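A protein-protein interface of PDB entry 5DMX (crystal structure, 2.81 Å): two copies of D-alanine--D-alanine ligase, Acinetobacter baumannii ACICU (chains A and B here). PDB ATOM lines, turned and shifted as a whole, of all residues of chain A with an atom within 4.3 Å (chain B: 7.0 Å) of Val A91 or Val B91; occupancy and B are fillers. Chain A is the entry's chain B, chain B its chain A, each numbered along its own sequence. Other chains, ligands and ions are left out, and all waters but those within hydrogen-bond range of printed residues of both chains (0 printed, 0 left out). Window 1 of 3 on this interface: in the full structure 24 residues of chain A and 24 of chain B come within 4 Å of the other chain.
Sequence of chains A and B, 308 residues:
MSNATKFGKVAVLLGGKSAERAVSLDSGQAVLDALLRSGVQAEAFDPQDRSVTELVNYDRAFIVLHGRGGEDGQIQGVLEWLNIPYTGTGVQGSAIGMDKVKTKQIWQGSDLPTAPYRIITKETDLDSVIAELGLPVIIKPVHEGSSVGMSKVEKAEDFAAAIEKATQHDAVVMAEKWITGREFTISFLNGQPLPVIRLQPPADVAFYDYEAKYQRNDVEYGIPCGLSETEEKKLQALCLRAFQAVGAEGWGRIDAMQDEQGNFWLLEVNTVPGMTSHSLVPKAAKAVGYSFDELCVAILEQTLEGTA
The side-chain amide nitrogen of Gln B92 sits at hydrogen-bond distance from the backbone carbonyl oxygen of Ala A95.
O of Ala B95 sits at hydrogen-bond distance from NE2 of Gln A92.
The side-chain carboxylate (OD1) of Asp B72 lies within hydrogen-bond range of the backbone NH (N) of Gln B74 (3.3 Å).
OE2 of Glu A80 lies within hydrogen-bond range of OH of Tyr A86, 3.1 Å away.
Among the printed residues, pairs that only touch across the chains: Val A91 with Val B91, Glu A80 with Gln B74 and Gly A77 with Gln B74.
Of chain B, only Val B91 comes within 4 Å of Val A91.
Of chain A, only Val A91 comes within 4 Å of Val B91.
Of the printed residues of chain B, Gln A92 touches Ala B95 (3.2 Å).
Printed residues of chain B within 4 Å of Glu A80: Gln B74.
Printed residues of chain A within 4 Å of Gln B74: Gly A77 and Glu A80.
Of the printed residues of chain A, Gln B92 touches Ala A95.
Tyr B86 touches none of the printed residues of chain A.
The nearest printed residue of chain A that does not touch Val B91 is Ala A95 (4.3 Å).
Hydrophobic or aromatic side chains of chain A within 4 Å of the printed part of chain B: Val A91 and Ala A95.
Of the 20 printed residues of chain B, 4 touch a printed residue of chain A.
Hydrophobic or aromatic side chains of chain B within 4 Å of the printed part of chain A: Val B91 and Ala B95.
Among the printed residues, 5 pairs touch across the chains.
Val B91 touches its own counterpart, Val A91.
Gln A92 touches Ala B95, and with the chains exchanged Ala A95 touches Gln B92.
11 positions are printed for both chains.
Of the 5 pairs that touch across the chains among the printed residues, 3 have their exchanged pair printed and touching as well.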
ATOM      1  N   GLY A  73      -8.974  29.013  14.168  1.00  0.00           N
ATOM      2  CA  GLY A  73      -7.549  29.242  14.500  1.00  0.00           C
ATOM      3  C   GLY A  73      -6.477  28.425  13.761  1.00  0.00           C
ATOM      4  O   GLY A  73      -5.345  28.884  13.648  1.00  0.00           O
ATOM      5  N   GLN A  76      -5.105  30.149  10.590  1.00  0.00           N
ATOM      6  CA  GLN A  76      -4.504  31.391  11.096  1.00  0.00           C
ATOM      7  C   GLN A  76      -3.137  31.071  11.661  1.00  0.00           C
ATOM      8  O   GLN A  76      -2.180  31.820  11.467  1.00  0.00           O
ATOM      9  CB  GLN A  76      -5.337  32.043  12.213  1.00  0.00           C
ATOM     10  CG  GLN A  76      -6.649  32.701  11.811  1.00  0.00           C
ATOM     11  CD  GLN A  76      -7.751  31.729  11.455  1.00  0.00           C
ATOM     12  OE1 GLN A  76      -7.661  30.524  11.714  1.00  0.00           O
ATOM     13  NE2 GLN A  76      -8.740  32.226  10.735  1.00  0.00           N
ATOM     14  N   GLY A  77      -3.052  29.924  12.328  1.00  0.00           N
ATOM     15  CA  GLY A  77      -1.793  29.373  12.749  1.00  0.00           C
ATOM     16  C   GLY A  77      -0.785  29.299  11.613  1.00  0.00           C
ATOM     17  O   GLY A  77       0.280  29.914  11.723  1.00  0.00           O
ATOM     18  N   GLU A  80       0.520  32.539  10.368  1.00  0.00           N
ATOM     19  CA  GLU A  80       1.428  33.230  11.305  1.00  0.00           C
ATOM     20  C   GLU A  80       2.821  32.658  11.130  1.00  0.00           C
ATOM     21  O   GLU A  80       3.789  33.396  10.979  1.00  0.00           O
ATOM     22  CB  GLU A  80       0.990  33.087  12.764  1.00  0.00           C
ATOM     23  CG  GLU A  80      -0.325  33.747  13.140  1.00  0.00           C
ATOM     24  CD  GLU A  80      -0.246  35.249  13.320  1.00  0.00           C
ATOM     25  OE1 GLU A  80       0.733  35.863  12.870  1.00  0.00           O
ATOM     26  OE2 GLU A  80      -1.198  35.824  13.895  1.00  0.00           O
ATOM     27  N   TYR A  86      -3.117  38.454   6.927  1.00  0.00           N
ATOM     28  CA  TYR A  86      -4.390  37.849   6.569  1.00  0.00           C
ATOM     29  C   TYR A  86      -5.609  38.538   7.183  1.00  0.00           C
ATOM     30  O   TYR A  86      -5.495  39.340   8.095  1.00  0.00           O
ATOM     31  CB  TYR A  86      -4.361  36.378   6.921  1.00  0.00           C
ATOM     32  CG  TYR A  86      -4.223  36.087   8.384  1.00  0.00           C
ATOM     33  CD1 TYR A  86      -5.332  36.091   9.222  1.00  0.00           C
ATOM     34  CD2 TYR A  86      -2.991  35.807   8.940  1.00  0.00           C
ATOM     35  CE1 TYR A  86      -5.214  35.849  10.582  1.00  0.00           C
ATOM     36  CE2 TYR A  86      -2.865  35.547  10.287  1.00  0.00           C
ATOM     37  CZ  TYR A  86      -3.972  35.576  11.102  1.00  0.00           C
ATOM     38  OH  TYR A  86      -3.822  35.312  12.424  1.00  0.00           O
ATOM     39  N   GLY A  90      -7.318  36.836  14.504  1.00  0.00           N
ATOM     40  CA  GLY A  90      -6.162  35.990  14.731  1.00  0.00           C
ATOM     41  C   GLY A  90      -6.475  34.657  15.389  1.00  0.00           C
ATOM     42  O   GLY A  90      -7.640  34.260  15.476  1.00  0.00           O
ATOM     43  N   VAL A  91      -5.436  33.976  15.893  1.00  0.00           N
ATOM     44  CA  VAL A  91      -5.592  32.570  16.343  1.00  0.00           C
ATOM     45  C   VAL A  91      -6.458  32.463  17.589  1.00  0.00           C
ATOM     46  O   VAL A  91      -7.332  31.604  17.672  1.00  0.00           O
ATOM     47  CB  VAL A  91      -4.250  31.877  16.646  1.00  0.00           C
ATOM     48  CG1 VAL A  91      -4.479  30.412  16.981  1.00  0.00           C
ATOM     49  CG2 VAL A  91      -3.308  31.998  15.454  1.00  0.00           C
ATOM     50  N   GLN A  92      -6.244  33.380  18.521  1.00  0.00           N
ATOM     51  CA  GLN A  92      -6.968  33.378  19.778  1.00  0.00           C
ATOM     52  C   GLN A  92      -8.466  33.582  19.592  1.00  0.00           C
ATOM     53  O   GLN A  92      -9.260  32.706  19.952  1.00  0.00           O
ATOM     54  CB  GLN A  92      -6.397  34.445  20.687  1.00  0.00           C
ATOM     55  CG  GLN A  92      -6.830  34.324  22.123  1.00  0.00           C
ATOM     56  CD  GLN A  92      -6.530  35.595  22.862  1.00  0.00           C
ATOM     57  OE1 GLN A  92      -7.249  36.589  22.710  1.00  0.00           O
ATOM     58  NE2 GLN A  92      -5.468  35.588  23.654  1.00  0.00           N
ATOM     59  N   GLY A  93      -8.845  34.717  19.005  1.00  0.00           N
ATOM     60  CA  GLY A  93     -10.262  35.059  18.792  1.00  0.00           C
ATOM     61  C   GLY A  93     -11.015  34.027  17.966  1.00  0.00           C
ATOM     62  O   GLY A  93     -12.166  33.720  18.250  1.00  0.00           O
ATOM     63  N   SER A  94     -10.346  33.461  16.971  1.00  0.00           N
ATOM     64  CA  SER A  94     -10.929  32.425  16.154  1.00  0.00           C
ATOM     65  C   SER A  94     -11.214  31.188  16.963  1.00  0.00           C
ATOM     66  O   SER A  94     -12.323  30.660  16.925  1.00  0.00           O
ATOM     67  CB  SER A  94      -9.996  32.094  15.002  1.00  0.00           C
ATOM     68  OG  SER A  94      -9.632  33.302  14.350  1.00  0.00           O
ATOM     69  N   ALA A  95     -10.211  30.717  17.698  1.00  0.00           N
ATOM     70  CA  ALA A  95     -10.311  29.462  18.470  1.00  0.00           C
ATOM     71  C   ALA A  95     -11.380  29.510  19.555  1.00  0.00           C
ATOM     72  O   ALA A  95     -12.081  28.507  19.771  1.00  0.00           O
ATOM     73  CB  ALA A  95      -8.975  29.127  19.097  1.00  0.00           C
ATOM     74  N   GLU B  71       3.730  28.320  22.658  1.00  0.00           N
ATOM     75  CA  GLU B  71       2.833  28.296  23.823  1.00  0.00           C
ATOM     76  C   GLU B  71       1.471  28.921  23.458  1.00  0.00           C
ATOM     77  O   GLU B  71       0.569  28.934  24.299  1.00  0.00           O
ATOM     78  CB  GLU B  71       3.488  29.035  25.056  1.00  0.00           C
ATOM     79  CG  GLU B  71       4.046  28.188  26.254  1.00  0.00           C
ATOM     80  CD  GLU B  71       4.852  28.984  27.335  1.00  0.00           C
ATOM     81  OE1 GLU B  71       4.396  29.099  28.501  1.00  0.00           O
ATOM     82  OE2 GLU B  71       5.960  29.529  27.063  1.00  0.00           O
ATOM     83  N   ASP B  72       1.304  29.412  22.219  1.00  0.00           N
ATOM     84  CA  ASP B  72       0.170  30.306  21.855  1.00  0.00           C
ATOM     85  C   ASP B  72      -0.774  29.856  20.720  1.00  0.00           C
ATOM     86  O   ASP B  72      -1.580  30.666  20.242  1.00  0.00           O
ATOM     87  CB  ASP B  72       0.702  31.707  21.510  1.00  0.00           C
ATOM     88  CG  ASP B  72       1.448  31.742  20.202  1.00  0.00           C
ATOM     89  OD1 ASP B  72       1.524  30.695  19.541  1.00  0.00           O
ATOM     90  OD2 ASP B  72       1.986  32.817  19.838  1.00  0.00           O
ATOM     91  N   GLY B  73      -0.694  28.596  20.296  1.00  0.00           N
ATOM     92  CA  GLY B  73      -1.626  28.062  19.284  1.00  0.00           C
ATOM     93  C   GLY B  73      -1.135  27.990  17.839  1.00  0.00           C
ATOM     94  O   GLY B  73      -1.677  27.211  17.059  1.00  0.00           O
ATOM     95  N   GLN B  74      -0.119  28.772  17.487  1.00  0.00           N
ATOM     96  CA  GLN B  74       0.369  28.837  16.113  1.00  0.00           C
ATOM     97  C   GLN B  74       0.867  27.491  15.577  1.00  0.00           C
ATOM     98  O   GLN B  74       0.317  26.976  14.608  1.00  0.00           O
ATOM     99  CB  GLN B  74       1.474  29.869  15.970  1.00  0.00           C
ATOM    100  CG  GLN B  74       1.007  31.269  16.249  1.00  0.00           C
ATOM    101  CD  GLN B  74       2.103  32.289  16.080  1.00  0.00           C
ATOM    102  OE1 GLN B  74       3.107  32.060  15.384  1.00  0.00           O
ATOM    103  NE2 GLN B  74       1.890  33.471  16.640  1.00  0.00           N
ATOM    104  N   ILE B  75       1.892  26.917  16.197  1.00  0.00           N
ATOM    105  CA  ILE B  75       2.420  25.635  15.728  1.00  0.00           C
ATOM    106  C   ILE B  75       1.350  24.536  15.835  1.00  0.00           C
ATOM    107  O   ILE B  75       1.362  23.602  15.037  1.00  0.00           O
ATOM    108  CB  ILE B  75       3.733  25.200  16.461  1.00  0.00           C
ATOM    109  CG1 ILE B  75       4.475  24.112  15.668  1.00  0.00           C
ATOM    110  CG2 ILE B  75       3.466  24.704  17.882  1.00  0.00           C
ATOM    111  CD1 ILE B  75       5.064  24.594  14.366  1.00  0.00           C
ATOM    112  N   GLN B  76       0.446  24.654  16.813  1.00  0.00           N
ATOM    113  CA  GLN B  76      -0.633  23.685  16.982  1.00  0.00           C
ATOM    114  C   GLN B  76      -1.540  23.750  15.763  1.00  0.00           C
ATOM    115  O   GLN B  76      -2.029  22.728  15.285  1.00  0.00           O
ATOM    116  CB  GLN B  76      -1.486  23.958  18.235  1.00  0.00           C
ATOM    117  CG  GLN B  76      -0.819  23.680  19.567  1.00  0.00           C
ATOM    118  CD  GLN B  76       0.293  24.646  19.906  1.00  0.00           C
ATOM    119  OE1 GLN B  76       0.364  25.760  19.395  1.00  0.00           O
ATOM    120  NE2 GLN B  76       1.154  24.233  20.823  1.00  0.00           N
ATOM    121  N   GLY B  77      -1.771  24.967  15.287  1.00  0.00           N
ATOM    122  CA  GLY B  77      -2.478  25.189  14.061  1.00  0.00           C
ATOM    123  C   GLY B  77      -1.891  24.387  12.933  1.00  0.00           C
ATOM    124  O   GLY B  77      -2.607  23.573  12.343  1.00  0.00           O
ATOM    125  N   VAL B  78      -0.586  24.559  12.677  1.00  0.00           N
ATOM    126  CA  VAL B  78       0.030  23.916  11.504  1.00  0.00           C
ATOM    127  C   VAL B  78      -0.055  22.398  11.631  1.00  0.00           C
ATOM    128  O   VAL B  78      -0.285  21.711  10.643  1.00  0.00           O
ATOM    129  CB  VAL B  78       1.460  24.385  11.106  1.00  0.00           C
ATOM    130  CG1 VAL B  78       1.784  25.779  11.608  1.00  0.00           C
ATOM    131  CG2 VAL B  78       2.536  23.406  11.521  1.00  0.00           C
ATOM    132  N   GLU B  80      -2.385  20.676  13.146  1.00  0.00           N
ATOM    133  CA  GLU B  80      -3.774  20.262  12.862  1.00  0.00           C
ATOM    134  C   GLU B  80      -3.984  20.186  11.346  1.00  0.00           C
ATOM    135  O   GLU B  80      -4.480  19.189  10.843  1.00  0.00           O
ATOM    136  CB  GLU B  80      -4.814  21.218  13.475  1.00  0.00           C
ATOM    137  CG  GLU B  80      -4.832  21.305  14.993  1.00  0.00           C
ATOM    138  CD  GLU B  80      -5.495  20.139  15.682  1.00  0.00           C
ATOM    139  OE1 GLU B  80      -5.688  19.084  15.048  1.00  0.00           O
ATOM    140  OE2 GLU B  80      -5.805  20.269  16.885  1.00  0.00           O
ATOM    141  N   TYR B  86       0.089  15.500  18.288  1.00  0.00           N
ATOM    142  CA  TYR B  86       1.093  16.256  19.007  1.00  0.00           C
ATOM    143  C   TYR B  86       0.829  16.377  20.503  1.00  0.00           C
ATOM    144  O   TYR B  86      -0.261  16.139  20.979  1.00  0.00           O
ATOM    145  CB  TYR B  86       1.250  17.618  18.353  1.00  0.00           C
ATOM    146  CG  TYR B  86       0.024  18.466  18.393  1.00  0.00           C
ATOM    147  CD1 TYR B  86      -0.980  18.333  17.446  1.00  0.00           C
ATOM    148  CD2 TYR B  86      -0.143  19.407  19.381  1.00  0.00           C
ATOM    149  CE1 TYR B  86      -2.119  19.119  17.497  1.00  0.00           C
ATOM    150  CE2 TYR B  86      -1.266  20.197  19.438  1.00  0.00           C
ATOM    151  CZ  TYR B  86      -2.243  20.057  18.496  1.00  0.00           C
ATOM    152  OH  TYR B  86      -3.329  20.877  18.559  1.00  0.00           O
ATOM    153  N   THR B  89      -1.451  20.806  24.703  1.00  0.00           N
ATOM    154  CA  THR B  89      -2.708  21.512  24.602  1.00  0.00           C
ATOM    155  C   THR B  89      -2.951  21.932  23.154  1.00  0.00           C
ATOM    156  O   THR B  89      -2.017  22.358  22.470  1.00  0.00           O
ATOM    157  CB  THR B  89      -2.642  22.714  25.550  1.00  0.00           C
ATOM    158  OG1 THR B  89      -2.573  22.209  26.887  1.00  0.00           O
ATOM    159  CG2 THR B  89      -3.820  23.649  25.404  1.00  0.00           C
ATOM    160  N   GLY B  90      -4.198  21.787  22.699  1.00  0.00           N
ATOM    161  CA  GLY B  90      -4.591  22.195  21.362  1.00  0.00           C
ATOM    162  C   GLY B  90      -4.610  23.704  21.152  1.00  0.00           C
ATOM    163  O   GLY B  90      -4.083  24.462  21.963  1.00  0.00           O
ATOM    164  N   VAL B  91      -5.235  24.147  20.063  1.00  0.00           N
ATOM    165  CA  VAL B  91      -5.088  25.545  19.622  1.00  0.00           C
ATOM    166  C   VAL B  91      -5.766  26.497  20.586  1.00  0.00           C
ATOM    167  O   VAL B  91      -5.226  27.553  20.905  1.00  0.00           O
ATOM    168  CB  VAL B  91      -5.651  25.803  18.203  1.00  0.00           C
ATOM    169  CG1 VAL B  91      -5.365  27.237  17.755  1.00  0.00           C
ATOM    170  CG2 VAL B  91      -5.049  24.825  17.203  1.00  0.00           C
ATOM    171  N   GLN B  92      -6.958  26.118  21.027  1.00  0.00           N
ATOM    172  CA  GLN B  92      -7.762  26.966  21.882  1.00  0.00           C
ATOM    173  C   GLN B  92      -7.073  27.223  23.223  1.00  0.00           C
ATOM    174  O   GLN B  92      -6.769  28.377  23.555  1.00  0.00           O
ATOM    175  CB  GLN B  92      -9.113  26.327  22.089  1.00  0.00           C
ATOM    176  CG  GLN B  92     -10.125  27.257  22.705  1.00  0.00           C
ATOM    177  CD  GLN B  92     -11.300  26.475  23.219  1.00  0.00           C
ATOM    178  OE1 GLN B  92     -11.218  25.841  24.275  1.00  0.00           O
ATOM    179  NE2 GLN B  92     -12.391  26.483  22.476  1.00  0.00           N
ATOM    180  N   GLY B  93      -6.781  26.146  23.957  1.00  0.00           N
ATOM    181  CA  GLY B  93      -6.139  26.244  25.280  1.00  0.00           C
ATOM    182  C   GLY B  93      -4.802  26.963  25.263  1.00  0.00           C
ATOM    183  O   GLY B  93      -4.500  27.740  26.161  1.00  0.00           O
ATOM    184  N   SER B  94      -4.027  26.736  24.214  1.00  0.00           N
ATOM    185  CA  SER B  94      -2.758  27.399  24.035  1.00  0.00           C
ATOM    186  C   SER B  94      -2.943  28.892  23.859  1.00  0.00           C
ATOM    187  O   SER B  94      -2.302  29.670  24.549  1.00  0.00           O
ATOM    188  CB  SER B  94      -2.024  26.807  22.832  1.00  0.00           C
ATOM    189  OG  SER B  94      -2.014  25.397  22.964  1.00  0.00           O
ATOM    190  N   ALA B  95      -3.806  29.278  22.930  1.00  0.00           N
ATOM    191  CA  ALA B  95      -4.011  30.677  22.587  1.00  0.00           C
ATOM    192  C   ALA B  95      -4.517  31.510  23.764  1.00  0.00           C
ATOM    193  O   ALA B  95      -4.122  32.685  23.923  1.00  0.00           O
ATOM    194  CB  ALA B  95      -4.985  30.786  21.427  1.00  0.00           C
ATOM    195  N   ILE B  96      -5.404  30.900  24.552  1.00  0.00           N
ATOM    196  CA  ILE B  96      -5.912  31.497  25.783  1.00  0.00           C
ATOM    197  C   ILE B  96      -4.814  31.556  26.837  1.00  0.00           C
ATOM    198  O   ILE B  96      -4.492  32.642  27.321  1.00  0.00           O
ATOM    199  CB  ILE B  96      -7.081  30.687  26.374  1.00  0.00           C
ATOM    200  CG1 ILE B  96      -8.314  30.756  25.477  1.00  0.00           C
ATOM    201  CG2 ILE B  96      -7.435  31.196  27.758  1.00  0.00           C
ATOM    202  CD1 ILE B  96      -9.370  29.745  25.836  1.00  0.00           C
ATOM    203  N   GLY B  97      -4.244  30.389  27.153  1.00  0.00           N
ATOM    204  CA  GLY B  97      -3.222  30.231  28.187  1.00  0.00           C
ATOM    205  C   GLY B  97      -2.106  31.259  28.199  1.00  0.00           C
ATOM    206  O   GLY B  97      -1.644  31.682  29.246  1.00  0.00           O
ATOM    207  N   GLU B 249      -4.694  20.363  28.131  1.00  0.00           N
ATOM    208  CA  GLU B 249      -4.691  18.899  28.247  1.00  0.00           C
ATOM    209  C   GLU B 249      -3.302  18.296  28.194  1.00  0.00           C
ATOM    210  O   GLU B 249      -2.402  18.860  27.615  1.00  0.00           O
ATOM    211  CB  GLU B 249      -5.642  18.271  27.210  1.00  0.00           C
ATOM    212  CG  GLU B 249      -5.458  18.768  25.778  1.00  0.00           C
ATOM    213  CD  GLU B 249      -6.716  18.762  24.891  1.00  0.00           C
ATOM    214  OE1 GLU B 249      -7.549  17.818  24.993  1.00  0.00           O
ATOM    215  OE2 GLU B 249      -6.844  19.717  24.069  1.00  0.00           O
